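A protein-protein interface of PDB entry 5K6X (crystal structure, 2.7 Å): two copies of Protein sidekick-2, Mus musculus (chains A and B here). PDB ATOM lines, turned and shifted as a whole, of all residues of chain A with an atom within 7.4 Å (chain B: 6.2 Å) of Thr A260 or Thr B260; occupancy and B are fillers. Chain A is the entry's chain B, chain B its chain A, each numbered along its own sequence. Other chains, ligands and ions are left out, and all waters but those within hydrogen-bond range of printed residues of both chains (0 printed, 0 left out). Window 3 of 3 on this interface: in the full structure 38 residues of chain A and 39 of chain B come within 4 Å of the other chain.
Among the printed residues, merely in contact across the chains: Ala A213 with Gly B214 (3.6 Å), Gly A214 with Ala B213 (3.8 Å), Thr A260 with Thr B260 (3.9 Å), Thr A260 with Glu B291 (3.7 Å), Glu A291 with Asn B258 (3.1 Å) and Gln A294 with Asn B258 (3.5 Å).
The side-chain amide oxygen of Gln A294 lies close to the backbone carbonyl oxygen of Ala B257 (3.3 Å).
Ala A213 touches Gly B214, and with the chains exchanged Gly A214 touches Ala B213. Thr A260 touches its own counterpart, Thr B260. Thr A260 touches Glu B291, but with the chains exchanged Glu A291 does not touch Thr B260 (4.4 Å). Glu A291 touches Asn B258, but with the chains exchanged Asn A258 does not touch Glu B291 (4.1 Å). Positions printed for both chains: 213, 214, 256, 257, 258, 259, 260, 261, 262, 263, 264, 289 and 291. Of the 7 pairs that touch across the chains among the printed residues, 3 have their exchanged pair printed and touching as well.
The backbone NH of Thr B260 sits at hydrogen-bond distance from the side-chain carboxylate of Asp B263 (3.0 Å). O of Asn A258 sits at hydrogen-bond distance from OG1 of Thr A260 (3.4 Å). The backbone NH of Ala A213 is in hydrogen-bond range of the backbone carbonyl oxygen of Leu A290, 2.9 Å away. OD2 of Asp A263 sits at hydrogen-bond distance from N of Thr A260 (3.1 Å). The backbone carbonyl oxygen (O) of Asn B258 lies within hydrogen-bond range of the side-chain hydroxyl (OG1) of Thr B260 (3.3 Å). The backbone NH of Gly B214 is in hydrogen-bond range of the backbone carbonyl oxygen of Pro B259, at 3.3 Å.
Of the 13 printed residues of chain B, 6 touch a printed residue of chain A. Hydrophobic or aromatic side chains of chain B within 4 Å of the printed part of chain A: Ala B257. Among the printed residues, 7 pairs touch across the chains.
Val A212 touches none of the printed residues of chain B. Thr A260 touches just these residues of chain B: Thr B260 and Glu B291. Leu A287 touches none of the printed residues of chain B. Of the printed residues of chain B, Glu A291 touches Asn B258. Of the printed residues of chain A, Ala B257 touches Gln A294. Printed residues of chain A within 4 Å of Asn B258: Glu A291 (3.1 Å) and Gln A294 (3.5 Å). Of chain A, only Thr A260 comes within 4 Å of Thr B260. Of the printed residues of chain A, Glu B291 touches Thr A260.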
ATOM      1  N   VAL A 211     -14.969  17.072 -22.835  1.00  0.00           N
ATOM      2  CA  VAL A 211     -14.400  16.288 -21.751  1.00  0.00           C
ATOM      3  C   VAL A 211     -13.617  15.106 -22.323  1.00  0.00           C
ATOM      4  O   VAL A 211     -13.920  14.617 -23.411  1.00  0.00           O
ATOM      5  CB  VAL A 211     -15.504  15.797 -20.777  1.00  0.00           C
ATOM      6  CG1 VAL A 211     -16.260  14.608 -21.356  1.00  0.00           C
ATOM      7  CG2 VAL A 211     -14.913  15.452 -19.428  1.00  0.00           C
ATOM      8  N   VAL A 212     -12.589  14.671 -21.605  1.00  0.00           N
ATOM      9  CA  VAL A 212     -11.808  13.516 -22.026  1.00  0.00           C
ATOM     10  C   VAL A 212     -12.375  12.267 -21.358  1.00  0.00           C
ATOM     11  O   VAL A 212     -12.796  12.319 -20.203  1.00  0.00           O
ATOM     12  CB  VAL A 212     -10.313  13.689 -21.676  1.00  0.00           C
ATOM     13  CG1 VAL A 212      -9.528  12.435 -22.019  1.00  0.00           C
ATOM     14  CG2 VAL A 212      -9.734  14.886 -22.413  1.00  0.00           C
ATOM     15  N   ALA A 213     -12.405  11.155 -22.086  1.00  0.00           N
ATOM     16  CA  ALA A 213     -12.934   9.906 -21.548  1.00  0.00           C
ATOM     17  C   ALA A 213     -12.172   9.482 -20.292  1.00  0.00           C
ATOM     18  O   ALA A 213     -10.943   9.456 -20.283  1.00  0.00           O
ATOM     19  CB  ALA A 213     -12.877   8.808 -22.600  1.00  0.00           C
ATOM     20  N   GLY A 214     -12.911   9.155 -19.236  1.00  0.00           N
ATOM     21  CA  GLY A 214     -12.311   8.749 -17.977  1.00  0.00           C
ATOM     22  C   GLY A 214     -12.143   9.870 -16.965  1.00  0.00           C
ATOM     23  O   GLY A 214     -11.512   9.682 -15.925  1.00  0.00           O
ATOM     24  N   VAL A 218     -18.858  14.704 -15.770  1.00  0.00           N
ATOM     25  CA  VAL A 218     -19.108  15.888 -16.584  1.00  0.00           C
ATOM     26  C   VAL A 218     -20.581  16.274 -16.452  1.00  0.00           C
ATOM     27  O   VAL A 218     -21.462  15.411 -16.450  1.00  0.00           O
ATOM     28  CB  VAL A 218     -18.729  15.660 -18.067  1.00  0.00           C
ATOM     29  CG1 VAL A 218     -19.533  14.515 -18.673  1.00  0.00           C
ATOM     30  CG2 VAL A 218     -18.900  16.943 -18.870  1.00  0.00           C
ATOM     31  N   LYS A 238     -30.979  12.923 -24.435  1.00  0.00           N
ATOM     32  CA  LYS A 238     -29.742  12.759 -25.186  1.00  0.00           C
ATOM     33  C   LYS A 238     -30.082  12.268 -26.583  1.00  0.00           C
ATOM     34  O   LYS A 238     -30.571  11.149 -26.749  1.00  0.00           O
ATOM     35  CB  LYS A 238     -28.797  11.774 -24.502  1.00  0.00           C
ATOM     36  CG  LYS A 238     -27.530  11.503 -25.298  1.00  0.00           C
ATOM     37  CD  LYS A 238     -26.814  10.254 -24.813  1.00  0.00           C
ATOM     38  CE  LYS A 238     -25.538  10.015 -25.605  1.00  0.00           C
ATOM     39  NZ  LYS A 238     -25.790  10.015 -27.071  1.00  0.00           N
ATOM     40  N   ILE A 256     -23.040  13.012 -16.024  1.00  0.00           N
ATOM     41  CA  ILE A 256     -22.679  11.713 -16.575  1.00  0.00           C
ATOM     42  C   ILE A 256     -21.417  11.178 -15.920  1.00  0.00           C
ATOM     43  O   ILE A 256     -20.330  11.720 -16.121  1.00  0.00           O
ATOM     44  CB  ILE A 256     -22.455  11.786 -18.091  1.00  0.00           C
ATOM     45  CG1 ILE A 256     -23.716  12.288 -18.790  1.00  0.00           C
ATOM     46  CG2 ILE A 256     -22.037  10.425 -18.633  1.00  0.00           C
ATOM     47  CD1 ILE A 256     -23.595  12.313 -20.280  1.00  0.00           C
ATOM     48  N   ALA A 257     -21.561  10.119 -15.131  1.00  0.00           N
ATOM     49  CA  ALA A 257     -20.405   9.485 -14.517  1.00  0.00           C
ATOM     50  C   ALA A 257     -19.668   8.641 -15.548  1.00  0.00           C
ATOM     51  O   ALA A 257     -20.292   7.946 -16.352  1.00  0.00           O
ATOM     52  CB  ALA A 257     -20.826   8.635 -13.331  1.00  0.00           C
ATOM     53  N   ASN A 258     -18.340   8.708 -15.509  1.00  0.00           N
ATOM     54  CA  ASN A 258     -17.484   7.937 -16.406  1.00  0.00           C
ATOM     55  C   ASN A 258     -17.845   8.104 -17.883  1.00  0.00           C
ATOM     56  O   ASN A 258     -18.182   7.124 -18.551  1.00  0.00           O
ATOM     57  CB  ASN A 258     -17.532   6.455 -16.030  1.00  0.00           C
ATOM     58  CG  ASN A 258     -17.412   6.233 -14.539  1.00  0.00           C
ATOM     59  OD1 ASN A 258     -16.661   6.928 -13.855  1.00  0.00           O
ATOM     60  ND2 ASN A 258     -18.157   5.260 -14.024  1.00  0.00           N
ATOM     61  N   PRO A 259     -17.793   9.344 -18.396  1.00  0.00           N
ATOM     62  CA  PRO A 259     -18.233   9.580 -19.775  1.00  0.00           C
ATOM     63  C   PRO A 259     -17.354   8.877 -20.810  1.00  0.00           C
ATOM     64  O   PRO A 259     -16.130   8.857 -20.679  1.00  0.00           O
ATOM     65  CB  PRO A 259     -18.130  11.102 -19.919  1.00  0.00           C
ATOM     66  CG  PRO A 259     -17.094  11.501 -18.929  1.00  0.00           C
ATOM     67  CD  PRO A 259     -17.260  10.567 -17.770  1.00  0.00           C
ATOM     68  N   THR A 260     -17.991   8.312 -21.831  1.00  0.00           N
ATOM     69  CA  THR A 260     -17.293   7.614 -22.904  1.00  0.00           C
ATOM     70  C   THR A 260     -17.699   8.275 -24.217  1.00  0.00           C
ATOM     71  O   THR A 260     -18.609   9.102 -24.231  1.00  0.00           O
ATOM     72  CB  THR A 260     -17.630   6.108 -22.924  1.00  0.00           C
ATOM     73  OG1 THR A 260     -17.748   5.626 -21.581  1.00  0.00           O
ATOM     74  CG2 THR A 260     -16.553   5.309 -23.657  1.00  0.00           C
ATOM     75  N   VAL A 261     -17.022   7.937 -25.312  1.00  0.00           N
ATOM     76  CA  VAL A 261     -17.361   8.488 -26.622  1.00  0.00           C
ATOM     77  C   VAL A 261     -18.823   8.224 -26.987  1.00  0.00           C
ATOM     78  O   VAL A 261     -19.426   8.979 -27.747  1.00  0.00           O
ATOM     79  CB  VAL A 261     -16.446   7.924 -27.729  1.00  0.00           C
ATOM     80  CG1 VAL A 261     -15.011   8.365 -27.503  1.00  0.00           C
ATOM     81  CG2 VAL A 261     -16.546   6.405 -27.797  1.00  0.00           C
ATOM     82  N   SER A 262     -19.384   7.149 -26.442  1.00  0.00           N
ATOM     83  CA  SER A 262     -20.792   6.836 -26.637  1.00  0.00           C
ATOM     84  C   SER A 262     -21.687   7.835 -25.903  1.00  0.00           C
ATOM     85  O   SER A 262     -22.836   8.047 -26.288  1.00  0.00           O
ATOM     86  CB  SER A 262     -21.091   5.412 -26.166  1.00  0.00           C
ATOM     87  OG  SER A 262     -20.777   5.257 -24.793  1.00  0.00           O
ATOM     88  N   ASP A 263     -21.155   8.446 -24.847  1.00  0.00           N
ATOM     89  CA  ASP A 263     -21.911   9.408 -24.052  1.00  0.00           C
ATOM     90  C   ASP A 263     -21.942  10.784 -24.711  1.00  0.00           C
ATOM     91  O   ASP A 263     -22.543  11.718 -24.185  1.00  0.00           O
ATOM     92  CB  ASP A 263     -21.329   9.519 -22.641  1.00  0.00           C
ATOM     93  CG  ASP A 263     -21.749   8.371 -21.745  1.00  0.00           C
ATOM     94  OD1 ASP A 263     -22.908   7.922 -21.855  1.00  0.00           O
ATOM     95  OD2 ASP A 263     -20.921   7.920 -20.927  1.00  0.00           O
ATOM     96  N   ALA A 264     -21.292  10.906 -25.862  1.00  0.00           N
ATOM     97  CA  ALA A 264     -21.268  12.165 -26.589  1.00  0.00           C
ATOM     98  C   ALA A 264     -22.552  12.318 -27.393  1.00  0.00           C
ATOM     99  O   ALA A 264     -23.214  11.330 -27.706  1.00  0.00           O
ATOM    100  CB  ALA A 264     -20.053  12.236 -27.497  1.00  0.00           C
ATOM    101  N   GLY A 265     -22.903  13.554 -27.726  1.00  0.00           N
ATOM    102  CA  GLY A 265     -24.107  13.807 -28.494  1.00  0.00           C
ATOM    103  C   GLY A 265     -24.788  15.110 -28.133  1.00  0.00           C
ATOM    104  O   GLY A 265     -24.225  15.942 -27.423  1.00  0.00           O
ATOM    105  N   TYR A 267     -27.342  17.057 -26.077  1.00  0.00           N
ATOM    106  CA  TYR A 267     -28.142  17.027 -24.860  1.00  0.00           C
ATOM    107  C   TYR A 267     -29.023  18.265 -24.796  1.00  0.00           C
ATOM    108  O   TYR A 267     -28.526  19.391 -24.826  1.00  0.00           O
ATOM    109  CB  TYR A 267     -27.246  16.937 -23.627  1.00  0.00           C
ATOM    110  CG  TYR A 267     -26.544  15.607 -23.498  1.00  0.00           C
ATOM    111  CD1 TYR A 267     -27.049  14.610 -22.676  1.00  0.00           C
ATOM    112  CD2 TYR A 267     -25.381  15.341 -24.209  1.00  0.00           C
ATOM    113  CE1 TYR A 267     -26.412  13.392 -22.555  1.00  0.00           C
ATOM    114  CE2 TYR A 267     -24.740  14.126 -24.098  1.00  0.00           C
ATOM    115  CZ  TYR A 267     -25.260  13.155 -23.270  1.00  0.00           C
ATOM    116  OH  TYR A 267     -24.624  11.941 -23.159  1.00  0.00           O
ATOM    117  N   LEU A 287     -22.230  17.587 -26.142  1.00  0.00           N
ATOM    118  CA  LEU A 287     -21.207  17.061 -25.252  1.00  0.00           C
ATOM    119  C   LEU A 287     -20.159  16.358 -26.093  1.00  0.00           C
ATOM    120  O   LEU A 287     -20.457  15.383 -26.783  1.00  0.00           O
ATOM    121  CB  LEU A 287     -21.797  16.096 -24.226  1.00  0.00           C
ATOM    122  CG  LEU A 287     -20.768  15.461 -23.289  1.00  0.00           C
ATOM    123  CD1 LEU A 287     -20.082  16.524 -22.442  1.00  0.00           C
ATOM    124  CD2 LEU A 287     -21.404  14.395 -22.411  1.00  0.00           C
ATOM    125  N   SER A 288     -18.932  16.859 -26.045  1.00  0.00           N
ATOM    126  CA  SER A 288     -17.847  16.244 -26.788  1.00  0.00           C
ATOM    127  C   SER A 288     -16.948  15.448 -25.857  1.00  0.00           C
ATOM    128  O   SER A 288     -16.177  16.017 -25.086  1.00  0.00           O
ATOM    129  CB  SER A 288     -17.037  17.305 -27.531  1.00  0.00           C
ATOM    130  OG  SER A 288     -17.869  18.062 -28.391  1.00  0.00           O
ATOM    131  N   VAL A 289     -17.056  14.126 -25.933  1.00  0.00           N
ATOM    132  CA  VAL A 289     -16.174  13.256 -25.173  1.00  0.00           C
ATOM    133  C   VAL A 289     -14.965  12.944 -26.041  1.00  0.00           C
ATOM    134  O   VAL A 289     -15.103  12.478 -27.172  1.00  0.00           O
ATOM    135  CB  VAL A 289     -16.866  11.960 -24.736  1.00  0.00           C
ATOM    136  CG1 VAL A 289     -15.908  11.112 -23.916  1.00  0.00           C
ATOM    137  CG2 VAL A 289     -18.114  12.280 -23.930  1.00  0.00           C
ATOM    138  N   LEU A 290     -13.780  13.203 -25.504  1.00  0.00           N
ATOM    139  CA  LEU A 290     -12.563  13.173 -26.300  1.00  0.00           C
ATOM    140  C   LEU A 290     -11.678  11.977 -25.982  1.00  0.00           C
ATOM    141  O   LEU A 290     -11.577  11.548 -24.833  1.00  0.00           O
ATOM    142  CB  LEU A 290     -11.778  14.469 -26.092  1.00  0.00           C
ATOM    143  CG  LEU A 290     -12.589  15.759 -26.237  1.00  0.00           C
ATOM    144  CD1 LEU A 290     -11.703  16.982 -26.044  1.00  0.00           C
ATOM    145  CD2 LEU A 290     -13.293  15.808 -27.584  1.00  0.00           C
ATOM    146  N   GLU A 291     -11.041  11.441 -27.018  1.00  0.00           N
ATOM    147  CA  GLU A 291     -10.034  10.407 -26.842  1.00  0.00           C
ATOM    148  C   GLU A 291      -8.712  10.866 -27.440  1.00  0.00           C
ATOM    149  O   GLU A 291      -8.653  11.232 -28.614  1.00  0.00           O
ATOM    150  CB  GLU A 291     -10.479   9.096 -27.496  1.00  0.00           C
ATOM    151  CG  GLU A 291     -11.512   8.298 -26.703  1.00  0.00           C
ATOM    152  CD  GLU A 291     -10.925   7.542 -25.524  1.00  0.00           C
ATOM    153  OE1 GLU A 291     -11.529   6.528 -25.115  1.00  0.00           O
ATOM    154  OE2 GLU A 291      -9.870   7.955 -24.998  1.00  0.00           O
ATOM    155  N   GLN A 294      -4.107   7.735 -30.776  1.00  0.00           N
ATOM    156  CA  GLN A 294      -3.461   6.435 -30.666  1.00  0.00           C
ATOM    157  C   GLN A 294      -3.056   5.977 -32.064  1.00  0.00           C
ATOM    158  O   GLN A 294      -3.818   6.118 -33.023  1.00  0.00           O
ATOM    159  CB  GLN A 294      -4.369   5.413 -29.975  1.00  0.00           C
ATOM    160  CG  GLN A 294      -5.367   4.694 -30.862  1.00  0.00           C
ATOM    161  CD  GLN A 294      -6.215   3.702 -30.090  1.00  0.00           C
ATOM    162  OE1 GLN A 294      -7.080   4.088 -29.305  1.00  0.00           O
ATOM    163  NE2 GLN A 294      -5.965   2.414 -30.305  1.00  0.00           N
ATOM    164  N   ALA B 213     -11.178   2.237 -17.239  1.00  0.00           N
ATOM    165  CA  ALA B 213     -11.423   2.897 -18.518  1.00  0.00           C
ATOM    166  C   ALA B 213     -10.961   4.353 -18.501  1.00  0.00           C
ATOM    167  O   ALA B 213     -11.289   5.109 -17.588  1.00  0.00           O
ATOM    168  CB  ALA B 213     -12.899   2.815 -18.878  1.00  0.00           C
ATOM    169  N   GLY B 214     -10.199   4.740 -19.521  1.00  0.00           N
ATOM    170  CA  GLY B 214      -9.688   6.095 -19.627  1.00  0.00           C
ATOM    171  C   GLY B 214      -8.290   6.283 -19.066  1.00  0.00           C
ATOM    172  O   GLY B 214      -7.804   7.410 -18.966  1.00  0.00           O
ATOM    173  N   ILE B 256      -2.608  -1.207 -25.283  1.00  0.00           N
ATOM    174  CA  ILE B 256      -3.908  -0.694 -25.684  1.00  0.00           C
ATOM    175  C   ILE B 256      -4.096   0.727 -25.178  1.00  0.00           C
ATOM    176  O   ILE B 256      -4.251   0.958 -23.979  1.00  0.00           O
ATOM    177  CB  ILE B 256      -5.048  -1.578 -25.160  1.00  0.00           C
ATOM    178  CG1 ILE B 256      -4.893  -3.002 -25.696  1.00  0.00           C
ATOM    179  CG2 ILE B 256      -6.399  -0.996 -25.551  1.00  0.00           C
ATOM    180  CD1 ILE B 256      -6.011  -3.921 -25.299  1.00  0.00           C
ATOM    181  N   ALA B 257      -4.079   1.678 -26.104  1.00  0.00           N
ATOM    182  CA  ALA B 257      -4.314   3.073 -25.766  1.00  0.00           C
ATOM    183  C   ALA B 257      -5.801   3.332 -25.556  1.00  0.00           C
ATOM    184  O   ALA B 257      -6.639   2.803 -26.289  1.00  0.00           O
ATOM    185  CB  ALA B 257      -3.760   3.982 -26.843  1.00  0.00           C
ATOM    186  N   ASN B 258      -6.110   4.150 -24.553  1.00  0.00           N
ATOM    187  CA  ASN B 258      -7.485   4.519 -24.235  1.00  0.00           C
ATOM    188  C   ASN B 258      -8.397   3.310 -24.047  1.00  0.00           C
ATOM    189  O   ASN B 258      -9.383   3.162 -24.772  1.00  0.00           O
ATOM    190  CB  ASN B 258      -8.053   5.420 -25.332  1.00  0.00           C
ATOM    191  CG  ASN B 258      -7.088   6.506 -25.748  1.00  0.00           C
ATOM    192  OD1 ASN B 258      -6.378   7.071 -24.917  1.00  0.00           O
ATOM    193  ND2 ASN B 258      -7.052   6.806 -27.043  1.00  0.00           N
ATOM    194  N   PRO B 259      -8.073   2.438 -23.075  1.00  0.00           N
ATOM    195  CA  PRO B 259      -8.837   1.195 -22.932  1.00  0.00           C
ATOM    196  C   PRO B 259     -10.296   1.438 -22.556  1.00  0.00           C
ATOM    197  O   PRO B 259     -10.593   2.298 -21.727  1.00  0.00           O
ATOM    198  CB  PRO B 259      -8.099   0.459 -21.810  1.00  0.00           C
ATOM    199  CG  PRO B 259      -7.450   1.537 -21.019  1.00  0.00           C
ATOM    200  CD  PRO B 259      -7.063   2.591 -22.013  1.00  0.00           C
ATOM    201  N   THR B 260     -11.191   0.675 -23.173  1.00  0.00           N
ATOM    202  CA  THR B 260     -12.618   0.783 -22.907  1.00  0.00           C
ATOM    203  C   THR B 260     -13.115  -0.597 -22.490  1.00  0.00           C
ATOM    204  O   THR B 260     -12.389  -1.581 -22.625  1.00  0.00           O
ATOM    205  CB  THR B 260     -13.390   1.287 -24.146  1.00  0.00           C
ATOM    206  OG1 THR B 260     -12.608   2.271 -24.833  1.00  0.00           O
ATOM    207  CG2 THR B 260     -14.734   1.891 -23.750  1.00  0.00           C
ATOM    208  N   VAL B 261     -14.339  -0.674 -21.974  1.00  0.00           N
ATOM    209  CA  VAL B 261     -14.926  -1.953 -21.588  1.00  0.00           C
ATOM    210  C   VAL B 261     -14.964  -2.924 -22.771  1.00  0.00           C
ATOM    211  O   VAL B 261     -14.920  -4.142 -22.590  1.00  0.00           O
ATOM    212  CB  VAL B 261     -16.348  -1.771 -21.015  1.00  0.00           C
ATOM    213  CG1 VAL B 261     -16.300  -0.970 -19.723  1.00  0.00           C
ATOM    214  CG2 VAL B 261     -17.262  -1.101 -22.033  1.00  0.00           C
ATOM    215  N   SER B 262     -15.036  -2.374 -23.979  1.00  0.00           N
ATOM    216  CA  SER B 262     -15.010  -3.166 -25.201  1.00  0.00           C
ATOM    217  C   SER B 262     -13.635  -3.783 -25.446  1.00  0.00           C
ATOM    218  O   SER B 262     -13.517  -4.801 -26.125  1.00  0.00           O
ATOM    219  CB  SER B 262     -15.418  -2.306 -26.400  1.00  0.00           C
ATOM    220  OG  SER B 262     -14.539  -1.205 -26.557  1.00  0.00           O
ATOM    221  N   ASP B 263     -12.601  -3.159 -24.889  1.00  0.00           N
ATOM    222  CA  ASP B 263     -11.231  -3.627 -25.073  1.00  0.00           C
ATOM    223  C   ASP B 263     -10.903  -4.805 -24.160  1.00  0.00           C
ATOM    224  O   ASP B 263      -9.792  -5.331 -24.190  1.00  0.00           O
ATOM    225  CB  ASP B 263     -10.240  -2.489 -24.819  1.00  0.00           C
ATOM    226  CG  ASP B 263     -10.140  -1.531 -25.988  1.00  0.00           C
ATOM    227  OD1 ASP B 263     -10.197  -1.993 -27.146  1.00  0.00           O
ATOM    228  OD2 ASP B 263     -10.004  -0.313 -25.748  1.00  0.00           O
ATOM    229  N   ALA B 264     -11.873  -5.215 -23.350  1.00  0.00           N
ATOM    230  CA  ALA B 264     -11.682  -6.337 -22.441  1.00  0.00           C
ATOM    231  C   ALA B 264     -11.870  -7.659 -23.176  1.00  0.00           C
ATOM    232  O   ALA B 264     -12.526  -7.713 -24.217  1.00  0.00           O
ATOM    233  CB  ALA B 264     -12.642  -6.238 -21.266  1.00  0.00           C
ATOM    234  N   VAL B 289     -11.100  -4.493 -18.036  1.00  0.00           N
ATOM    235  CA  VAL B 289     -11.278  -3.048 -18.037  1.00  0.00           C
ATOM    236  C   VAL B 289     -12.414  -2.667 -17.095  1.00  0.00           C
ATOM    237  O   VAL B 289     -13.533  -3.162 -17.224  1.00  0.00           O
ATOM    238  CB  VAL B 289     -11.569  -2.507 -19.445  1.00  0.00           C
ATOM    239  CG1 VAL B 289     -11.727  -0.996 -19.403  1.00  0.00           C
ATOM    240  CG2 VAL B 289     -10.454  -2.903 -20.401  1.00  0.00           C
ATOM    241  N   GLU B 291     -14.936   0.002 -14.813  1.00  0.00           N
ATOM    242  CA  GLU B 291     -15.610   1.286 -14.664  1.00  0.00           C
ATOM    243  C   GLU B 291     -16.180   1.408 -13.259  1.00  0.00           C
ATOM    244  O   GLU B 291     -16.933   0.539 -12.814  1.00  0.00           O
ATOM    245  CB  GLU B 291     -16.718   1.460 -15.707  1.00  0.00           C
ATOM    246  CG  GLU B 291     -16.214   1.858 -17.086  1.00  0.00           C
ATOM    247  CD  GLU B 291     -17.298   2.481 -17.944  1.00  0.00           C
ATOM    248  OE1 GLU B 291     -18.492   2.230 -17.675  1.00  0.00           O
ATOM    249  OE2 GLU B 291     -16.955   3.231 -18.881  1.00  0.00           O
